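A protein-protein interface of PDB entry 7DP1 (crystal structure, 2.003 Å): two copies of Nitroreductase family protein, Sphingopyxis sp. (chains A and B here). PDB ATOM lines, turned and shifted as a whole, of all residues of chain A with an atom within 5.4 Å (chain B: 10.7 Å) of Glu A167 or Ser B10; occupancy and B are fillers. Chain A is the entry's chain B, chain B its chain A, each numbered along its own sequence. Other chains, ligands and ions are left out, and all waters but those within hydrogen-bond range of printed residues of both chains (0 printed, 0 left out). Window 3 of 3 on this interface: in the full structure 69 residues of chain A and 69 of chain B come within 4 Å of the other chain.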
ATOM      1  N   LEU A   9     -14.373 -23.679   3.455  1.00  0.00           N
ATOM      2  CA  LEU A   9     -15.716 -23.780   4.030  1.00  0.00           C
ATOM      3  C   LEU A   9     -15.684 -24.135   5.525  1.00  0.00           C
ATOM      4  O   LEU A   9     -15.214 -25.213   5.907  1.00  0.00           O
ATOM      5  CB  LEU A   9     -16.540 -24.818   3.271  1.00  0.00           C
ATOM      6  CG  LEU A   9     -18.062 -24.714   3.398  1.00  0.00           C
ATOM      7  CD1 LEU A   9     -18.573 -23.476   2.661  1.00  0.00           C
ATOM      8  CD2 LEU A   9     -18.727 -25.975   2.878  1.00  0.00           C
ATOM      9  N   SER A  10     -16.222 -23.243   6.359  1.00  0.00           N
ATOM     10  CA  SER A  10     -16.185 -23.413   7.814  1.00  0.00           C
ATOM     11  C   SER A  10     -17.109 -24.512   8.309  1.00  0.00           C
ATOM     12  O   SER A  10     -18.131 -24.795   7.685  1.00  0.00           O
ATOM     13  CB  SER A  10     -16.581 -22.115   8.499  1.00  0.00           C
ATOM     14  OG  SER A  10     -17.994 -22.002   8.519  1.00  0.00           O
ATOM     15  N   ALA A  11     -16.770 -25.096   9.458  1.00  0.00           N
ATOM     16  CA  ALA A  11     -17.556 -26.182  10.035  1.00  0.00           C
ATOM     17  C   ALA A  11     -19.030 -25.798  10.222  1.00  0.00           C
ATOM     18  O   ALA A  11     -19.937 -26.613  10.005  1.00  0.00           O
ATOM     19  CB  ALA A  11     -16.952 -26.613  11.359  1.00  0.00           C
ATOM     20  N   ALA A  14     -20.507 -25.829   6.789  1.00  0.00           N
ATOM     21  CA  ALA A  14     -20.671 -27.217   6.365  1.00  0.00           C
ATOM     22  C   ALA A  14     -21.913 -27.795   7.013  1.00  0.00           C
ATOM     23  O   ALA A  14     -22.730 -28.428   6.349  1.00  0.00           O
ATOM     24  CB  ALA A  14     -19.449 -28.064   6.732  1.00  0.00           C
ATOM     25  N   LEU A 163     -20.048 -34.230   6.758  1.00  0.00           N
ATOM     26  CA  LEU A 163     -19.582 -32.843   6.720  1.00  0.00           C
ATOM     27  C   LEU A 163     -18.396 -32.641   5.802  1.00  0.00           C
ATOM     28  O   LEU A 163     -18.301 -31.623   5.117  1.00  0.00           O
ATOM     29  CB  LEU A 163     -19.222 -32.364   8.125  1.00  0.00           C
ATOM     30  CG  LEU A 163     -20.418 -32.304   9.077  1.00  0.00           C
ATOM     31  CD1 LEU A 163     -19.964 -31.828  10.471  1.00  0.00           C
ATOM     32  CD2 LEU A 163     -21.541 -31.435   8.512  1.00  0.00           C
ATOM     33  N   LEU A 164     -17.470 -33.601   5.800  1.00  0.00           N
ATOM     34  CA  LEU A 164     -16.300 -33.507   4.933  1.00  0.00           C
ATOM     35  C   LEU A 164     -16.696 -33.551   3.470  1.00  0.00           C
ATOM     36  O   LEU A 164     -16.050 -32.920   2.638  1.00  0.00           O
ATOM     37  CB  LEU A 164     -15.293 -34.610   5.257  1.00  0.00           C
ATOM     38  CG  LEU A 164     -14.458 -34.381   6.526  1.00  0.00           C
ATOM     39  CD1 LEU A 164     -13.819 -35.669   7.026  1.00  0.00           C
ATOM     40  CD2 LEU A 164     -13.370 -33.388   6.214  1.00  0.00           C
ATOM     41  N   LEU A 165     -17.758 -34.299   3.156  1.00  0.00           N
ATOM     42  CA  LEU A 165     -18.239 -34.416   1.773  1.00  0.00           C
ATOM     43  C   LEU A 165     -18.691 -33.053   1.238  1.00  0.00           C
ATOM     44  O   LEU A 165     -18.302 -32.640   0.149  1.00  0.00           O
ATOM     45  CB  LEU A 165     -19.385 -35.443   1.687  1.00  0.00           C
ATOM     46  CG  LEU A 165     -18.964 -36.910   1.813  1.00  0.00           C
ATOM     47  CD1 LEU A 165     -20.167 -37.858   1.904  1.00  0.00           C
ATOM     48  CD2 LEU A 165     -18.090 -37.293   0.617  1.00  0.00           C
ATOM     49  N   VAL A 166     -19.545 -32.381   2.011  1.00  0.00           N
ATOM     50  CA  VAL A 166     -20.016 -31.030   1.696  1.00  0.00           C
ATOM     51  C   VAL A 166     -18.872 -30.028   1.497  1.00  0.00           C
ATOM     52  O   VAL A 166     -18.852 -29.254   0.537  1.00  0.00           O
ATOM     53  CB  VAL A 166     -20.948 -30.526   2.830  1.00  0.00           C
ATOM     54  CG1 VAL A 166     -21.054 -29.017   2.833  1.00  0.00           C
ATOM     55  CG2 VAL A 166     -22.326 -31.209   2.731  1.00  0.00           C
ATOM     56  N   GLU A 167     -17.916 -30.048   2.415  1.00  0.00           N
ATOM     57  CA  GLU A 167     -16.735 -29.176   2.326  1.00  0.00           C
ATOM     58  C   GLU A 167     -15.938 -29.360   1.044  1.00  0.00           C
ATOM     59  O   GLU A 167     -15.306 -28.441   0.532  1.00  0.00           O
ATOM     60  CB  GLU A 167     -15.821 -29.420   3.532  1.00  0.00           C
ATOM     61  CG  GLU A 167     -14.591 -28.512   3.576  1.00  0.00           C
ATOM     62  CD  GLU A 167     -13.647 -28.877   4.700  1.00  0.00           C
ATOM     63  OE1 GLU A 167     -13.270 -30.063   4.824  1.00  0.00           O
ATOM     64  OE2 GLU A 167     -13.298 -27.977   5.485  1.00  0.00           O
ATOM     65  N   HIS A 168     -15.982 -30.586   0.554  1.00  0.00           N
ATOM     66  CA  HIS A 168     -15.220 -31.064  -0.602  1.00  0.00           C
ATOM     67  C   HIS A 168     -16.032 -31.116  -1.884  1.00  0.00           C
ATOM     68  O   HIS A 168     -15.602 -31.697  -2.890  1.00  0.00           O
ATOM     69  CB  HIS A 168     -14.675 -32.412  -0.169  1.00  0.00           C
ATOM     70  CG  HIS A 168     -13.561 -32.277   0.820  1.00  0.00           C
ATOM     71  ND1 HIS A 168     -13.097 -33.336   1.579  1.00  0.00           N
ATOM     72  CD2 HIS A 168     -12.597 -31.320   0.892  1.00  0.00           C
ATOM     73  CE1 HIS A 168     -12.038 -32.931   2.277  1.00  0.00           C
ATOM     74  NE2 HIS A 168     -11.707 -31.722   1.857  1.00  0.00           N
ATOM     75  N   GLY A 169     -17.175 -30.429  -1.872  1.00  0.00           N
ATOM     76  CA  GLY A 169     -17.986 -30.262  -3.071  1.00  0.00           C
ATOM     77  C   GLY A 169     -18.892 -31.452  -3.354  1.00  0.00           C
ATOM     78  O   GLY A 169     -19.528 -31.515  -4.402  1.00  0.00           O
ATOM     79  N   LEU B   9     -12.160 -21.165  10.343  1.00  0.00           N
ATOM     80  CA  LEU B   9     -11.697 -22.543  10.501  1.00  0.00           C
ATOM     81  C   LEU B   9     -12.547 -23.573   9.733  1.00  0.00           C
ATOM     82  O   LEU B   9     -13.744 -23.727   9.994  1.00  0.00           O
ATOM     83  CB  LEU B   9     -11.665 -22.925  11.982  1.00  0.00           C
ATOM     84  CG  LEU B   9     -10.764 -24.127  12.280  1.00  0.00           C
ATOM     85  CD1 LEU B   9      -9.324 -23.731  12.084  1.00  0.00           C
ATOM     86  CD2 LEU B   9     -10.980 -24.685  13.680  1.00  0.00           C
ATOM     87  N   SER B  10     -11.921 -24.285   8.800  1.00  0.00           N
ATOM     88  CA  SER B  10     -12.623 -25.267   7.957  1.00  0.00           C
ATOM     89  C   SER B  10     -12.991 -26.563   8.688  1.00  0.00           C
ATOM     90  O   SER B  10     -12.359 -26.930   9.673  1.00  0.00           O
ATOM     91  CB  SER B  10     -11.767 -25.622   6.752  1.00  0.00           C
ATOM     92  OG  SER B  10     -10.809 -26.602   7.116  1.00  0.00           O
ATOM     93  N   ALA B  11     -14.009 -27.267   8.197  1.00  0.00           N
ATOM     94  CA  ALA B  11     -14.437 -28.520   8.822  1.00  0.00           C
ATOM     95  C   ALA B  11     -13.275 -29.527   8.949  1.00  0.00           C
ATOM     96  O   ALA B  11     -13.152 -30.216   9.965  1.00  0.00           O
ATOM     97  CB  ALA B  11     -15.610 -29.133   8.042  1.00  0.00           C
ATOM     98  N   SER B  12     -12.415 -29.588   7.932  1.00  0.00           N
ATOM     99  CA  SER B  12     -11.230 -30.449   7.970  1.00  0.00           C
ATOM    100  C   SER B  12     -10.333 -30.113   9.145  1.00  0.00           C
ATOM    101  O   SER B  12      -9.870 -30.999   9.872  1.00  0.00           O
ATOM    102  CB  SER B  12     -10.417 -30.337   6.674  1.00  0.00           C
ATOM    103  OG  SER B  12     -11.126 -30.895   5.589  1.00  0.00           O
ATOM    104  N   GLU B  13     -10.072 -28.822   9.305  1.00  0.00           N
ATOM    105  CA  GLU B  13      -9.237 -28.321  10.389  1.00  0.00           C
ATOM    106  C   GLU B  13      -9.891 -28.549  11.738  1.00  0.00           C
ATOM    107  O   GLU B  13      -9.210 -28.850  12.714  1.00  0.00           O
ATOM    108  CB  GLU B  13      -8.938 -26.836  10.175  1.00  0.00           C
ATOM    109  CG  GLU B  13      -8.071 -26.590   8.937  1.00  0.00           C
ATOM    110  CD  GLU B  13      -8.211 -25.190   8.366  1.00  0.00           C
ATOM    111  OE1 GLU B  13      -9.115 -24.442   8.801  1.00  0.00           O
ATOM    112  OE2 GLU B  13      -7.412 -24.837   7.476  1.00  0.00           O
ATOM    113  N   ALA B  14     -11.216 -28.406  11.796  1.00  0.00           N
ATOM    114  CA  ALA B  14     -11.937 -28.669  13.027  1.00  0.00           C
ATOM    115  C   ALA B  14     -11.761 -30.128  13.425  1.00  0.00           C
ATOM    116  O   ALA B  14     -11.383 -30.415  14.556  1.00  0.00           O
ATOM    117  CB  ALA B  14     -13.433 -28.315  12.880  1.00  0.00           C
ATOM    118  N   LEU B  15     -12.020 -31.043  12.488  1.00  0.00           N
ATOM    119  CA  LEU B  15     -11.831 -32.479  12.729  1.00  0.00           C
ATOM    120  C   LEU B  15     -10.422 -32.797  13.221  1.00  0.00           C
ATOM    121  O   LEU B  15     -10.232 -33.605  14.140  1.00  0.00           O
ATOM    122  CB  LEU B  15     -12.088 -33.284  11.452  1.00  0.00           C
ATOM    123  CG  LEU B  15     -13.409 -34.032  11.239  1.00  0.00           C
ATOM    124  CD1 LEU B  15     -13.743 -34.884  12.465  1.00  0.00           C
ATOM    125  CD2 LEU B  15     -14.540 -33.081  10.914  1.00  0.00           C
ATOM    126  N   ALA B  16      -9.443 -32.172  12.573  1.00  0.00           N
ATOM    127  CA  ALA B  16      -8.039 -32.412  12.863  1.00  0.00           C
ATOM    128  C   ALA B  16      -7.650 -31.886  14.228  1.00  0.00           C
ATOM    129  O   ALA B  16      -6.918 -32.561  14.940  1.00  0.00           O
ATOM    130  CB  ALA B  16      -7.155 -31.794  11.792  1.00  0.00           C
ATOM    131  N   ARG B  17      -8.153 -30.707  14.612  1.00  0.00           N
ATOM    132  CA  ARG B  17      -7.719 -30.084  15.862  1.00  0.00           C
ATOM    133  C   ARG B  17      -8.576 -30.449  17.067  1.00  0.00           C
ATOM    134  O   ARG B  17      -8.213 -30.104  18.199  1.00  0.00           O
ATOM    135  CB  ARG B  17      -7.660 -28.549  15.732  1.00  0.00           C
ATOM    136  CG  ARG B  17      -6.777 -28.062  14.590  1.00  0.00           C
ATOM    137  CD  ARG B  17      -6.784 -26.550  14.378  1.00  0.00           C
ATOM    138  NE  ARG B  17      -5.499 -26.102  13.818  1.00  0.00           N
ATOM    139  CZ  ARG B  17      -5.319 -25.662  12.571  1.00  0.00           C
ATOM    140  NH1 ARG B  17      -6.342 -25.590  11.732  1.00  0.00           N
ATOM    141  NH2 ARG B  17      -4.110 -25.289  12.160  1.00  0.00           N
ATOM    142  N   ARG B  18      -9.700 -31.126  16.846  1.00  0.00           N
ATOM    143  CA  ARG B  18     -10.512 -31.603  17.969  1.00  0.00           C
ATOM    144  C   ARG B  18      -9.832 -32.776  18.669  1.00  0.00           C
ATOM    145  O   ARG B  18      -9.468 -33.758  18.036  1.00  0.00           O
ATOM    146  CB  ARG B  18     -11.922 -32.016  17.521  1.00  0.00           C
ATOM    147  CG  ARG B  18     -12.816 -32.457  18.718  1.00  0.00           C
ATOM    148  CD  ARG B  18     -13.672 -33.702  18.444  1.00  0.00           C
ATOM    149  NE  ARG B  18     -12.857 -34.836  18.011  1.00  0.00           N
ATOM    150  CZ  ARG B  18     -12.191 -35.649  18.823  1.00  0.00           C
ATOM    151  NH1 ARG B  18     -12.226 -35.449  20.135  1.00  0.00           N
ATOM    152  NH2 ARG B  18     -11.462 -36.652  18.310  1.00  0.00           N
ATOM    153  N   GLN B 159     -20.912 -35.097  17.926  1.00  0.00           N
ATOM    154  CA  GLN B 159     -19.758 -34.695  17.122  1.00  0.00           C
ATOM    155  C   GLN B 159     -19.970 -33.312  16.493  1.00  0.00           C
ATOM    156  O   GLN B 159     -19.029 -32.547  16.320  1.00  0.00           O
ATOM    157  CB  GLN B 159     -19.466 -35.732  16.023  1.00  0.00           C
ATOM    158  CG  GLN B 159     -18.369 -35.334  15.031  1.00  0.00           C
ATOM    159  CD  GLN B 159     -16.969 -35.374  15.636  1.00  0.00           C
ATOM    160  OE1 GLN B 159     -16.783 -35.256  16.868  1.00  0.00           O
ATOM    161  NE2 GLN B 159     -15.972 -35.539  14.779  1.00  0.00           N
ATOM    162  N   MET B 162     -18.970 -30.930  19.320  1.00  0.00           N
ATOM    163  CA  MET B 162     -17.544 -30.941  19.597  1.00  0.00           C
ATOM    164  C   MET B 162     -16.752 -30.186  18.516  1.00  0.00           C
ATOM    165  O   MET B 162     -15.799 -29.470  18.807  1.00  0.00           O
ATOM    166  CB  MET B 162     -17.067 -32.387  19.711  1.00  0.00           C
ATOM    167  CG  MET B 162     -17.602 -33.075  20.972  1.00  0.00           C
ATOM    168  SD  MET B 162     -16.840 -34.686  21.162  1.00  0.00           S
ATOM    169  CE  MET B 162     -17.849 -35.641  20.045  1.00  0.00           C
ATOM    170  N   LEU B 163     -17.148 -30.357  17.259  1.00  0.00           N
ATOM    171  CA  LEU B 163     -16.492 -29.617  16.185  1.00  0.00           C
ATOM    172  C   LEU B 163     -16.773 -28.122  16.244  1.00  0.00           C
ATOM    173  O   LEU B 163     -15.869 -27.326  16.020  1.00  0.00           O
ATOM    174  CB  LEU B 163     -16.925 -30.164  14.831  1.00  0.00           C
ATOM    175  CG  LEU B 163     -16.395 -31.579  14.583  1.00  0.00           C
ATOM    176  CD1 LEU B 163     -16.913 -32.114  13.270  1.00  0.00           C
ATOM    177  CD2 LEU B 163     -14.878 -31.518  14.590  1.00  0.00           C
ATOM    178  N   LEU B 164     -18.015 -27.744  16.563  1.00  0.00           N
ATOM    179  CA  LEU B 164     -18.364 -26.323  16.674  1.00  0.00           C
ATOM    180  C   LEU B 164     -17.597 -25.628  17.798  1.00  0.00           C
ATOM    181  O   LEU B 164     -17.248 -24.446  17.693  1.00  0.00           O
ATOM    182  CB  LEU B 164     -19.864 -26.161  16.919  1.00  0.00           C
ATOM    183  CG  LEU B 164     -20.710 -26.446  15.680  1.00  0.00           C
ATOM    184  CD1 LEU B 164     -22.199 -26.706  16.031  1.00  0.00           C
ATOM    185  CD2 LEU B 164     -20.575 -25.313  14.694  1.00  0.00           C
ATOM    186  N   LEU B 165     -17.355 -26.361  18.880  1.00  0.00           N
ATOM    187  CA  LEU B 165     -16.601 -25.821  20.001  1.00  0.00           C
ATOM    188  C   LEU B 165     -15.200 -25.455  19.562  1.00  0.00           C
ATOM    189  O   LEU B 165     -14.736 -24.336  19.773  1.00  0.00           O
ATOM    190  CB  LEU B 165     -16.546 -26.840  21.144  1.00  0.00           C
ATOM    191  CG  LEU B 165     -17.847 -27.036  21.928  1.00  0.00           C
ATOM    192  CD1 LEU B 165     -17.696 -28.188  22.915  1.00  0.00           C
ATOM    193  CD2 LEU B 165     -18.227 -25.737  22.659  1.00  0.00           C
ATOM    194  N   VAL B 166     -14.539 -26.420  18.927  1.00  0.00           N
ATOM    195  CA  VAL B 166     -13.183 -26.258  18.413  1.00  0.00           C
ATOM    196  C   VAL B 166     -13.099 -25.059  17.488  1.00  0.00           C
ATOM    197  O   VAL B 166     -12.170 -24.230  17.594  1.00  0.00           O
ATOM    198  CB  VAL B 166     -12.733 -27.525  17.665  1.00  0.00           C
ATOM    199  CG1 VAL B 166     -11.550 -27.236  16.758  1.00  0.00           C
ATOM    200  CG2 VAL B 166     -12.404 -28.633  18.662  1.00  0.00           C
ATOM    201  N   GLU B 167     -14.075 -24.965  16.594  1.00  0.00           N
ATOM    202  CA  GLU B 167     -14.181 -23.835  15.670  1.00  0.00           C
ATOM    203  C   GLU B 167     -14.264 -22.502  16.408  1.00  0.00           C
ATOM    204  O   GLU B 167     -13.757 -21.487  15.920  1.00  0.00           O
ATOM    205  CB  GLU B 167     -15.407 -23.992  14.767  1.00  0.00           C
ATOM    206  CG  GLU B 167     -15.575 -22.889  13.727  1.00  0.00           C
ATOM    207  CD  GLU B 167     -16.885 -22.996  12.959  1.00  0.00           C
ATOM    208  OE1 GLU B 167     -17.941 -23.120  13.610  1.00  0.00           O
ATOM    209  OE2 GLU B 167     -16.860 -22.945  11.709  1.00  0.00           O
ATOM    210  N   HIS B 168     -14.906 -22.489  17.572  1.00  0.00           N
ATOM    211  CA  HIS B 168     -15.053 -21.230  18.297  1.00  0.00           C
ATOM    212  C   HIS B 168     -14.043 -21.081  19.437  1.00  0.00           C
ATOM    213  O   HIS B 168     -14.198 -20.230  20.303  1.00  0.00           O
ATOM    214  CB  HIS B 168     -16.475 -21.073  18.838  1.00  0.00           C
ATOM    215  CG  HIS B 168     -17.511 -20.850  17.775  1.00  0.00           C
ATOM    216  ND1 HIS B 168     -18.115 -21.884  17.091  1.00  0.00           N
ATOM    217  CD2 HIS B 168     -18.053 -19.706  17.286  1.00  0.00           C
ATOM    218  CE1 HIS B 168     -18.987 -21.388  16.229  1.00  0.00           C
ATOM    219  NE2 HIS B 168     -18.965 -20.071  16.323  1.00  0.00           N
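Of chain B, only Ser B10 and Ala B11 come within 4 Å of Leu A9.
No residue of chain B comes within 4 Å of Ala A14.
Glu A167 touches three residues of chain B.
His A168 touches just one residue of chain B: Ser B12 (3.9 Å).
Of the printed residues of chain A, Ser B12 touches Leu A164 (3.4 Å), Glu A167 (2.4 Å) and His A168 (3.9 Å).
Of the printed residues of chain A, Glu B167 touches Ser A10 and Ala A11.
The nearest residue of chain B that does not touch Glu A167 is Glu B13 (5.1 Å).
The backbone carbonyl oxygen (O) of Leu B9 is in hydrogen-bond range of the backbone NH (N) of Ala A11 (3.4 Å).
The side-chain hydroxyl of Ser B10 lies close to the side-chain carboxylate of Glu A167 (3.3 Å).
The backbone NH (N) of Ala B11 sits at hydrogen-bond distance from the backbone carbonyl oxygen (O) of Leu A9 (3.3 Å).
OE2 of Glu A167 sits at hydrogen-bond distance from N of Ala B11 (2.9 Å).
The side-chain carboxylate (OE1) of Glu A167 is in hydrogen-bond range of the side-chain hydroxyl (OG) of Ser B12 (2.4 Å).
The side-chain carboxylate of Glu B167 sits at hydrogen-bond distance from the backbone NH of Ala A11 (3.1 Å).
OG of Ser B10 sits close to N of Ser B12, at 3.5 Å.
The backbone NH (N) of Ser B10 sits at hydrogen-bond distance from the side-chain carboxylate (OE1) of Glu B13 (2.8 Å).
O of Leu A164 sits close to ND1 of His A168 (3.2 Å).
Hydrophobic or aromatic side chains of chain B within 4 Å of the printed part of chain A: Ala B11.
Of the 11 printed residues of chain A, 6 touch a printed residue of chain B.
Hydrophobic or aromatic side chains of chain A that line the printed part of chain B: Ala A11, Leu A164 and His A168.
Among the printed residues, 12 pairs touch across the chains.
Among the printed residues, no Asp or Glu carboxylate lies within 4 Å of a Lys or Arg side-chain nitrogen of the other chain.
Leu A9 touches Ser B10, and with the chains exchanged Ser A10 touches Leu B9.
Ser A10 touches Glu B167, and with the chains exchanged Glu A167 touches Ser B10.
Ala A11 touches its own counterpart, Ala B11.
Ala A11 touches Glu B167, and with the chains exchanged Glu A167 touches Ala B11.
Among the printed residues, pairs that only touch across the chains: Leu A9 with Ser B10 (3.3 Å), Ser A10 with Leu B9 (3.3 Å), Ser A10 with Glu B167 (3.3 Å), Ala A11 with Ala B11 (3.7 Å), Leu A164 with Ser B12 (3.4 Å) and His A168 with Ser B12 (3.9 Å).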
